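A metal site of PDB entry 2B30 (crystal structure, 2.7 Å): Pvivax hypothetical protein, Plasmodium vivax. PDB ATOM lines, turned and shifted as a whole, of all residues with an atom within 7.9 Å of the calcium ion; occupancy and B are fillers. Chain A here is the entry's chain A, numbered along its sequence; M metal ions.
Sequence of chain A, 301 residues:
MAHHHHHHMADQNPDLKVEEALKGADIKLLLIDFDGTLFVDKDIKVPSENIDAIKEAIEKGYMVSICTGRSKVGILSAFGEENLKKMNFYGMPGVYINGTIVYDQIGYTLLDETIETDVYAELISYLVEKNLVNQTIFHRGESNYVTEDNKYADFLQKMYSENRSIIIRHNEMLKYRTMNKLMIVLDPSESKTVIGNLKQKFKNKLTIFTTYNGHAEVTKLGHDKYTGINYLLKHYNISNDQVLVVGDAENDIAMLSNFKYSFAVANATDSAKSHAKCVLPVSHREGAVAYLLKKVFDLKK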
ATOM      1  N   ILE A  32      15.374 -23.450  27.067  1.00  0.00           N
ATOM      2  CA  ILE A  32      15.950 -22.188  26.662  1.00  0.00           C
ATOM      3  C   ILE A  32      14.860 -21.182  26.407  1.00  0.00           C
ATOM      4  O   ILE A  32      13.972 -21.431  25.586  1.00  0.00           O
ATOM      5  CB  ILE A  32      16.750 -22.357  25.374  1.00  0.00           C
ATOM      6  CG1 ILE A  32      17.730 -23.534  25.506  1.00  0.00           C
ATOM      7  CG2 ILE A  32      17.468 -21.053  25.004  1.00  0.00           C
ATOM      8  CD1 ILE A  32      18.562 -23.796  24.253  1.00  0.00           C
ATOM      9  N   ASP A  33      14.900 -20.046  27.101  1.00  0.00           N
ATOM     10  CA  ASP A  33      13.979 -18.947  26.813  1.00  0.00           C
ATOM     11  C   ASP A  33      14.326 -18.331  25.458  1.00  0.00           C
ATOM     12  O   ASP A  33      15.476 -18.384  25.032  1.00  0.00           O
ATOM     13  CB  ASP A  33      14.039 -17.891  27.913  1.00  0.00           C
ATOM     14  CG  ASP A  33      13.144 -16.704  27.641  1.00  0.00           C
ATOM     15  OD1 ASP A  33      11.969 -16.878  27.245  1.00  0.00           O
ATOM     16  OD2 ASP A  33      13.617 -15.568  27.837  1.00  0.00           O
ATOM     17  N   PHE A  34      13.338 -17.768  24.779  1.00  0.00           N
ATOM     18  CA  PHE A  34      13.577 -17.168  23.465  1.00  0.00           C
ATOM     19  C   PHE A  34      13.991 -15.685  23.579  1.00  0.00           C
ATOM     20  O   PHE A  34      15.189 -15.394  23.575  1.00  0.00           O
ATOM     21  CB  PHE A  34      12.376 -17.376  22.520  1.00  0.00           C
ATOM     22  CG  PHE A  34      12.756 -17.285  21.058  1.00  0.00           C
ATOM     23  CD1 PHE A  34      13.542 -18.280  20.470  1.00  0.00           C
ATOM     24  CD2 PHE A  34      12.327 -16.220  20.268  1.00  0.00           C
ATOM     25  CE1 PHE A  34      13.897 -18.205  19.125  1.00  0.00           C
ATOM     26  CE2 PHE A  34      12.667 -16.136  18.914  1.00  0.00           C
ATOM     27  CZ  PHE A  34      13.460 -17.130  18.339  1.00  0.00           C
ATOM     28  N   ASP A  35      13.045 -14.763  23.706  1.00  0.00           N
ATOM     29  CA  ASP A  35      13.390 -13.338  23.687  1.00  0.00           C
ATOM     30  C   ASP A  35      14.108 -12.959  24.953  1.00  0.00           C
ATOM     31  O   ASP A  35      13.721 -13.386  26.044  1.00  0.00           O
ATOM     32  CB  ASP A  35      12.160 -12.453  23.565  1.00  0.00           C
ATOM     33  CG  ASP A  35      11.404 -12.686  22.301  1.00  0.00           C
ATOM     34  OD1 ASP A  35      10.795 -13.778  22.185  1.00  0.00           O
ATOM     35  OD2 ASP A  35      11.435 -11.799  21.426  1.00  0.00           O
ATOM     36  N   GLY A  36      15.148 -12.147  24.802  1.00  0.00           N
ATOM     37  CA  GLY A  36      15.956 -11.717  25.937  1.00  0.00           C
ATOM     38  C   GLY A  36      17.005 -12.730  26.326  1.00  0.00           C
ATOM     39  O   GLY A  36      17.903 -12.414  27.101  1.00  0.00           O
ATOM     40  N   THR A  37      16.911 -13.951  25.780  1.00  0.00           N
ATOM     41  CA  THR A  37      17.853 -15.017  26.086  1.00  0.00           C
ATOM     42  C   THR A  37      18.503 -15.475  24.788  1.00  0.00           C
ATOM     43  O   THR A  37      19.667 -15.181  24.554  1.00  0.00           O
ATOM     44  CB  THR A  37      17.156 -16.188  26.837  1.00  0.00           C
ATOM     45  OG1 THR A  37      16.558 -15.719  28.051  1.00  0.00           O
ATOM     46  CG2 THR A  37      18.154 -17.289  27.166  1.00  0.00           C
ATOM     47  N   LEU A  38      17.750 -16.163  23.942  1.00  0.00           N
ATOM     48  CA  LEU A  38      18.255 -16.693  22.678  1.00  0.00           C
ATOM     49  C   LEU A  38      18.096 -15.665  21.533  1.00  0.00           C
ATOM     50  O   LEU A  38      19.000 -15.495  20.720  1.00  0.00           O
ATOM     51  CB  LEU A  38      17.501 -17.982  22.340  1.00  0.00           C
ATOM     52  CG  LEU A  38      18.057 -18.911  21.255  1.00  0.00           C
ATOM     53  CD1 LEU A  38      19.349 -19.567  21.711  1.00  0.00           C
ATOM     54  CD2 LEU A  38      17.028 -19.980  20.896  1.00  0.00           C
ATOM     55  N   PHE A  39      16.954 -14.985  21.485  1.00  0.00           N
ATOM     56  CA  PHE A  39      16.648 -14.004  20.443  1.00  0.00           C
ATOM     57  C   PHE A  39      16.857 -12.600  20.982  1.00  0.00           C
ATOM     58  O   PHE A  39      16.249 -12.254  22.008  1.00  0.00           O
ATOM     59  CB  PHE A  39      15.201 -14.181  20.010  1.00  0.00           C
ATOM     60  CG  PHE A  39      14.761 -13.239  18.922  1.00  0.00           C
ATOM     61  CD1 PHE A  39      14.689 -13.657  17.596  1.00  0.00           C
ATOM     62  CD2 PHE A  39      14.392 -11.927  19.230  1.00  0.00           C
ATOM     63  CE1 PHE A  39      14.276 -12.798  16.607  1.00  0.00           C
ATOM     64  CE2 PHE A  39      13.976 -11.056  18.233  1.00  0.00           C
ATOM     65  CZ  PHE A  39      13.916 -11.495  16.912  1.00  0.00           C
ATOM     66  N   CYS A  67      11.207 -22.619  25.651  1.00  0.00           N
ATOM     67  CA  CYS A  67      10.086 -22.309  26.520  1.00  0.00           C
ATOM     68  C   CYS A  67       9.833 -20.806  26.420  1.00  0.00           C
ATOM     69  O   CYS A  67      10.676 -19.999  26.816  1.00  0.00           O
ATOM     70  CB  CYS A  67      10.426 -22.730  27.942  1.00  0.00           C
ATOM     71  SG  CYS A  67      10.998 -24.481  28.028  1.00  0.00           S
ATOM     72  N   THR A  68       8.676 -20.429  25.864  1.00  0.00           N
ATOM     73  CA  THR A  68       8.425 -19.028  25.552  1.00  0.00           C
ATOM     74  C   THR A  68       6.961 -18.656  25.559  1.00  0.00           C
ATOM     75  O   THR A  68       6.094 -19.528  25.501  1.00  0.00           O
ATOM     76  CB  THR A  68       8.999 -18.673  24.176  1.00  0.00           C
ATOM     77  OG1 THR A  68       8.912 -17.249  23.953  1.00  0.00           O
ATOM     78  CG2 THR A  68       8.250 -19.433  23.073  1.00  0.00           C
ATOM     79  N   GLY A  69       6.713 -17.350  25.599  1.00  0.00           N
ATOM     80  CA  GLY A  69       5.385 -16.787  25.411  1.00  0.00           C
ATOM     81  C   GLY A  69       4.912 -16.805  23.964  1.00  0.00           C
ATOM     82  O   GLY A  69       3.731 -16.660  23.702  1.00  0.00           O
ATOM     83  N   ARG A  70       5.836 -16.986  23.029  1.00  0.00           N
ATOM     84  CA  ARG A  70       5.488 -17.019  21.616  1.00  0.00           C
ATOM     85  C   ARG A  70       4.889 -18.348  21.211  1.00  0.00           C
ATOM     86  O   ARG A  70       4.901 -19.316  21.977  1.00  0.00           O
ATOM     87  CB  ARG A  70       6.715 -16.690  20.764  1.00  0.00           C
ATOM     88  CG  ARG A  70       7.083 -15.223  20.855  1.00  0.00           C
ATOM     89  CD  ARG A  70       8.524 -14.920  20.519  1.00  0.00           C
ATOM     90  NE  ARG A  70       8.717 -14.773  19.081  1.00  0.00           N
ATOM     91  CZ  ARG A  70       9.597 -13.963  18.494  1.00  0.00           C
ATOM     92  NH1 ARG A  70      10.419 -13.192  19.184  1.00  0.00           N
ATOM     93  NH2 ARG A  70       9.649 -13.931  17.172  1.00  0.00           N
ATOM     94  N   ASN A  98       3.414 -19.546  27.048  1.00  0.00           N
ATOM     95  CA  ASN A  98       3.530 -19.584  28.491  1.00  0.00           C
ATOM     96  C   ASN A  98       2.987 -20.848  29.127  1.00  0.00           C
ATOM     97  O   ASN A  98       2.428 -20.827  30.230  1.00  0.00           O
ATOM     98  CB  ASN A  98       2.915 -18.306  29.111  1.00  0.00           C
ATOM     99  CG  ASN A  98       3.790 -17.092  28.871  1.00  0.00           C
ATOM    100  OD1 ASN A  98       4.976 -17.237  28.540  1.00  0.00           O
ATOM    101  ND2 ASN A  98       3.233 -15.890  29.048  1.00  0.00           N
ATOM    102  N   THR A 211       5.498  -7.959  29.811  1.00  0.00           N
ATOM    103  CA  THR A 211       6.653  -8.145  28.911  1.00  0.00           C
ATOM    104  C   THR A 211       7.762  -7.201  29.348  1.00  0.00           C
ATOM    105  O   THR A 211       7.512  -6.253  30.108  1.00  0.00           O
ATOM    106  CB  THR A 211       6.259  -7.871  27.422  1.00  0.00           C
ATOM    107  OG1 THR A 211       5.202  -8.763  27.032  1.00  0.00           O
ATOM    108  CG2 THR A 211       7.416  -8.092  26.461  1.00  0.00           C
ATOM    109  N   TYR A 212       8.983  -7.487  28.889  1.00  0.00           N
ATOM    110  CA  TYR A 212      10.111  -6.582  29.073  1.00  0.00           C
ATOM    111  C   TYR A 212       9.849  -5.132  28.626  1.00  0.00           C
ATOM    112  O   TYR A 212      10.407  -4.205  29.193  1.00  0.00           O
ATOM    113  CB  TYR A 212      11.347  -7.128  28.341  1.00  0.00           C
ATOM    114  CG  TYR A 212      12.543  -6.217  28.434  1.00  0.00           C
ATOM    115  CD1 TYR A 212      13.275  -6.101  29.628  1.00  0.00           C
ATOM    116  CD2 TYR A 212      12.949  -5.456  27.336  1.00  0.00           C
ATOM    117  CE1 TYR A 212      14.371  -5.263  29.717  1.00  0.00           C
ATOM    118  CE2 TYR A 212      14.039  -4.620  27.412  1.00  0.00           C
ATOM    119  CZ  TYR A 212      14.747  -4.527  28.605  1.00  0.00           C
ATOM    120  OH  TYR A 212      15.828  -3.681  28.660  1.00  0.00           O
ATOM    121  N   GLU A 217       0.816  -9.907  28.553  1.00  0.00           N
ATOM    122  CA  GLU A 217       0.531 -11.215  27.994  1.00  0.00           C
ATOM    123  C   GLU A 217      -0.495 -11.904  28.889  1.00  0.00           C
ATOM    124  O   GLU A 217      -0.204 -12.167  30.055  1.00  0.00           O
ATOM    125  CB  GLU A 217       1.794 -12.071  27.906  1.00  0.00           C
ATOM    126  CG  GLU A 217       2.646 -11.799  26.677  1.00  0.00           C
ATOM    127  CD  GLU A 217       3.824 -12.756  26.532  1.00  0.00           C
ATOM    128  OE1 GLU A 217       4.456 -13.140  27.562  1.00  0.00           O
ATOM    129  OE2 GLU A 217       4.128 -13.143  25.377  1.00  0.00           O
ATOM    130  N   LYS A 225       5.271 -21.415  32.177  1.00  0.00           N
ATOM    131  CA  LYS A 225       6.280 -22.248  31.530  1.00  0.00           C
ATOM    132  C   LYS A 225       6.579 -23.498  32.350  1.00  0.00           C
ATOM    133  O   LYS A 225       6.655 -24.596  31.800  1.00  0.00           O
ATOM    134  CB  LYS A 225       7.574 -21.456  31.268  1.00  0.00           C
ATOM    135  CG  LYS A 225       7.456 -20.420  30.149  1.00  0.00           C
ATOM    136  CD  LYS A 225       8.811 -19.775  29.842  1.00  0.00           C
ATOM    137  CE  LYS A 225       8.664 -18.440  29.126  1.00  0.00           C
ATOM    138  NZ  LYS A 225       9.950 -17.959  28.537  1.00  0.00           N
ATOM    139  N   VAL A 246      17.416 -21.578  31.316  1.00  0.00           N
ATOM    140  CA  VAL A 246      17.976 -20.239  31.237  1.00  0.00           C
ATOM    141  C   VAL A 246      16.900 -19.226  30.782  1.00  0.00           C
ATOM    142  O   VAL A 246      16.104 -19.516  29.897  1.00  0.00           O
ATOM    143  CB  VAL A 246      19.284 -20.223  30.348  1.00  0.00           C
ATOM    144  CG1 VAL A 246      19.011 -20.624  28.922  1.00  0.00           C
ATOM    145  CG2 VAL A 246      19.969 -18.851  30.393  1.00  0.00           C
ATOM    146  N   GLY A 247      16.884 -18.044  31.397  1.00  0.00           N
ATOM    147  CA  GLY A 247      15.834 -17.059  31.139  1.00  0.00           C
ATOM    148  C   GLY A 247      16.139 -15.654  31.620  1.00  0.00           C
ATOM    149  O   GLY A 247      17.268 -15.360  32.010  1.00  0.00           O
ATOM    150  N   ASP A 248      15.143 -14.773  31.594  1.00  0.00           N
ATOM    151  CA  ASP A 248      15.407 -13.350  31.784  1.00  0.00           C
ATOM    152  C   ASP A 248      14.310 -12.507  32.419  1.00  0.00           C
ATOM    153  O   ASP A 248      14.612 -11.461  32.991  1.00  0.00           O
ATOM    154  CB  ASP A 248      15.764 -12.715  30.430  1.00  0.00           C
ATOM    155  CG  ASP A 248      14.568 -12.568  29.521  1.00  0.00           C
ATOM    156  OD1 ASP A 248      13.955 -13.593  29.185  1.00  0.00           O
ATOM    157  OD2 ASP A 248      14.227 -11.428  29.165  1.00  0.00           O
ATOM    158  N   ALA A 249      13.052 -12.941  32.327  1.00  0.00           N
ATOM    159  CA  ALA A 249      11.922 -12.073  32.617  1.00  0.00           C
ATOM    160  C   ALA A 249      10.923 -12.673  33.615  1.00  0.00           C
ATOM    161  O   ALA A 249      11.140 -13.748  34.187  1.00  0.00           O
ATOM    162  CB  ALA A 249      11.224 -11.729  31.306  1.00  0.00           C
ATOM    163  N   GLU A 250       9.814 -11.960  33.834  1.00  0.00           N
ATOM    164  CA  GLU A 250       8.765 -12.370  34.764  1.00  0.00           C
ATOM    165  C   GLU A 250       8.182 -13.760  34.454  1.00  0.00           C
ATOM    166  O   GLU A 250       7.912 -14.547  35.375  1.00  0.00           O
ATOM    167  CB  GLU A 250       7.648 -11.325  34.773  1.00  0.00           C
ATOM    168  CG  GLU A 250       6.730 -11.406  35.966  1.00  0.00           C
ATOM    169  CD  GLU A 250       5.699 -10.290  35.979  1.00  0.00           C
ATOM    170  OE1 GLU A 250       4.904 -10.186  35.015  1.00  0.00           O
ATOM    171  OE2 GLU A 250       5.684  -9.516  36.966  1.00  0.00           O
ATOM    172  N   ASN A 251       7.970 -14.064  33.170  1.00  0.00           N
ATOM    173  CA  ASN A 251       7.391 -15.348  32.774  1.00  0.00           C
ATOM    174  C   ASN A 251       8.375 -16.526  32.808  1.00  0.00           C
ATOM    175  O   ASN A 251       8.022 -17.645  32.414  1.00  0.00           O
ATOM    176  CB  ASN A 251       6.700 -15.239  31.406  1.00  0.00           C
ATOM    177  CG  ASN A 251       7.664 -14.972  30.289  1.00  0.00           C
ATOM    178  OD1 ASN A 251       8.751 -14.435  30.488  1.00  0.00           O
ATOM    179  ND2 ASN A 251       7.277 -15.359  29.078  1.00  0.00           N
ATOM    180  N   ASP A 252       9.603 -16.270  33.255  1.00  0.00           N
ATOM    181  CA  ASP A 252      10.617 -17.316  33.450  1.00  0.00           C
ATOM    182  C   ASP A 252      10.820 -17.677  34.927  1.00  0.00           C
ATOM    183  O   ASP A 252      11.491 -18.656  35.233  1.00  0.00           O
ATOM    184  CB  ASP A 252      11.982 -16.867  32.873  1.00  0.00           C
ATOM    185  CG  ASP A 252      11.941 -16.591  31.388  1.00  0.00           C
ATOM    186  OD1 ASP A 252      11.499 -17.479  30.629  1.00  0.00           O
ATOM    187  OD2 ASP A 252      12.369 -15.488  30.980  1.00  0.00           O
ATOM    188  N   MET A 255      10.160 -21.242  36.436  1.00  0.00           N
ATOM    189  CA  MET A 255      11.059 -22.284  35.963  1.00  0.00           C
ATOM    190  C   MET A 255      12.486 -22.052  36.440  1.00  0.00           C
ATOM    191  O   MET A 255      13.254 -23.008  36.574  1.00  0.00           O
ATOM    192  CB  MET A 255      10.998 -22.431  34.448  1.00  0.00           C
ATOM    193  CG  MET A 255      11.777 -21.402  33.664  1.00  0.00           C
ATOM    194  SD  MET A 255      11.636 -21.815  31.926  1.00  0.00           S
ATOM    195  CE  MET A 255      12.625 -20.519  31.180  1.00  0.00           C
ATOM    196  N   VAL A 265      20.390 -14.701  32.358  1.00  0.00           N
ATOM    197  CA  VAL A 265      21.325 -13.906  31.545  1.00  0.00           C
ATOM    198  C   VAL A 265      21.700 -12.613  32.267  1.00  0.00           C
ATOM    199  O   VAL A 265      20.947 -12.116  33.111  1.00  0.00           O
ATOM    200  CB  VAL A 265      20.748 -13.568  30.150  1.00  0.00           C
ATOM    201  CG1 VAL A 265      20.920 -14.728  29.191  1.00  0.00           C
ATOM    202  CG2 VAL A 265      19.284 -13.141  30.230  1.00  0.00           C
HETATM  203 CA    CA M   1      12.036 -14.050  27.501  1.00  0.00          CA
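The side-chain carboxylate (OD1) of Asp 33 sits close to the side-chain amino group (NZ) of Lys 225 (2.6 Å).
OG1 of Thr 37 lies close to OD2 of Asp 33, at 3.0 Å.
The backbone NH (N) of Leu 38 is in hydrogen-bond range of the backbone carbonyl oxygen (O) of Asp 33, at 3.4 Å.
O of Val 246 sits at hydrogen-bond distance from N of Asp 33 (3.1 Å).
The guanidinium group of Arg 70 lies within salt-bridge range of the side-chain carboxylate of Asp 35 (2.8 Å).
OD2 of Asp 252 sits at hydrogen-bond distance from N of Asp 248.
The side-chain carboxylate (OD2) of Asp 252 is in hydrogen-bond range of the backbone NH (N) of Ala 249 (3.0 Å).
NZ of Lys 225 lies within salt-bridge range of OD1 of Asp 252 (2.6 Å).
Merely in contact with the calcium ion: Asp 252 (3.8 Å).
Within 4 Å of the calcium ion: Asp 33, Asp 35, Asp 248 and Asp 252.
OD2 of Asp 33 binds the calcium ion, 2.2 Å away.
The calcium ion is bound by the backbone carbonyl oxygen (O) of Asp 35, 2.3 Å away.
The calcium ion is bound by the side-chain carboxylate (OD1) of Asp 248, at 2.6 Å.
The calcium ion is bound by OD1 of Asp 33 (2.8 Å).
The calcium ion has four donor atoms within binding distance.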
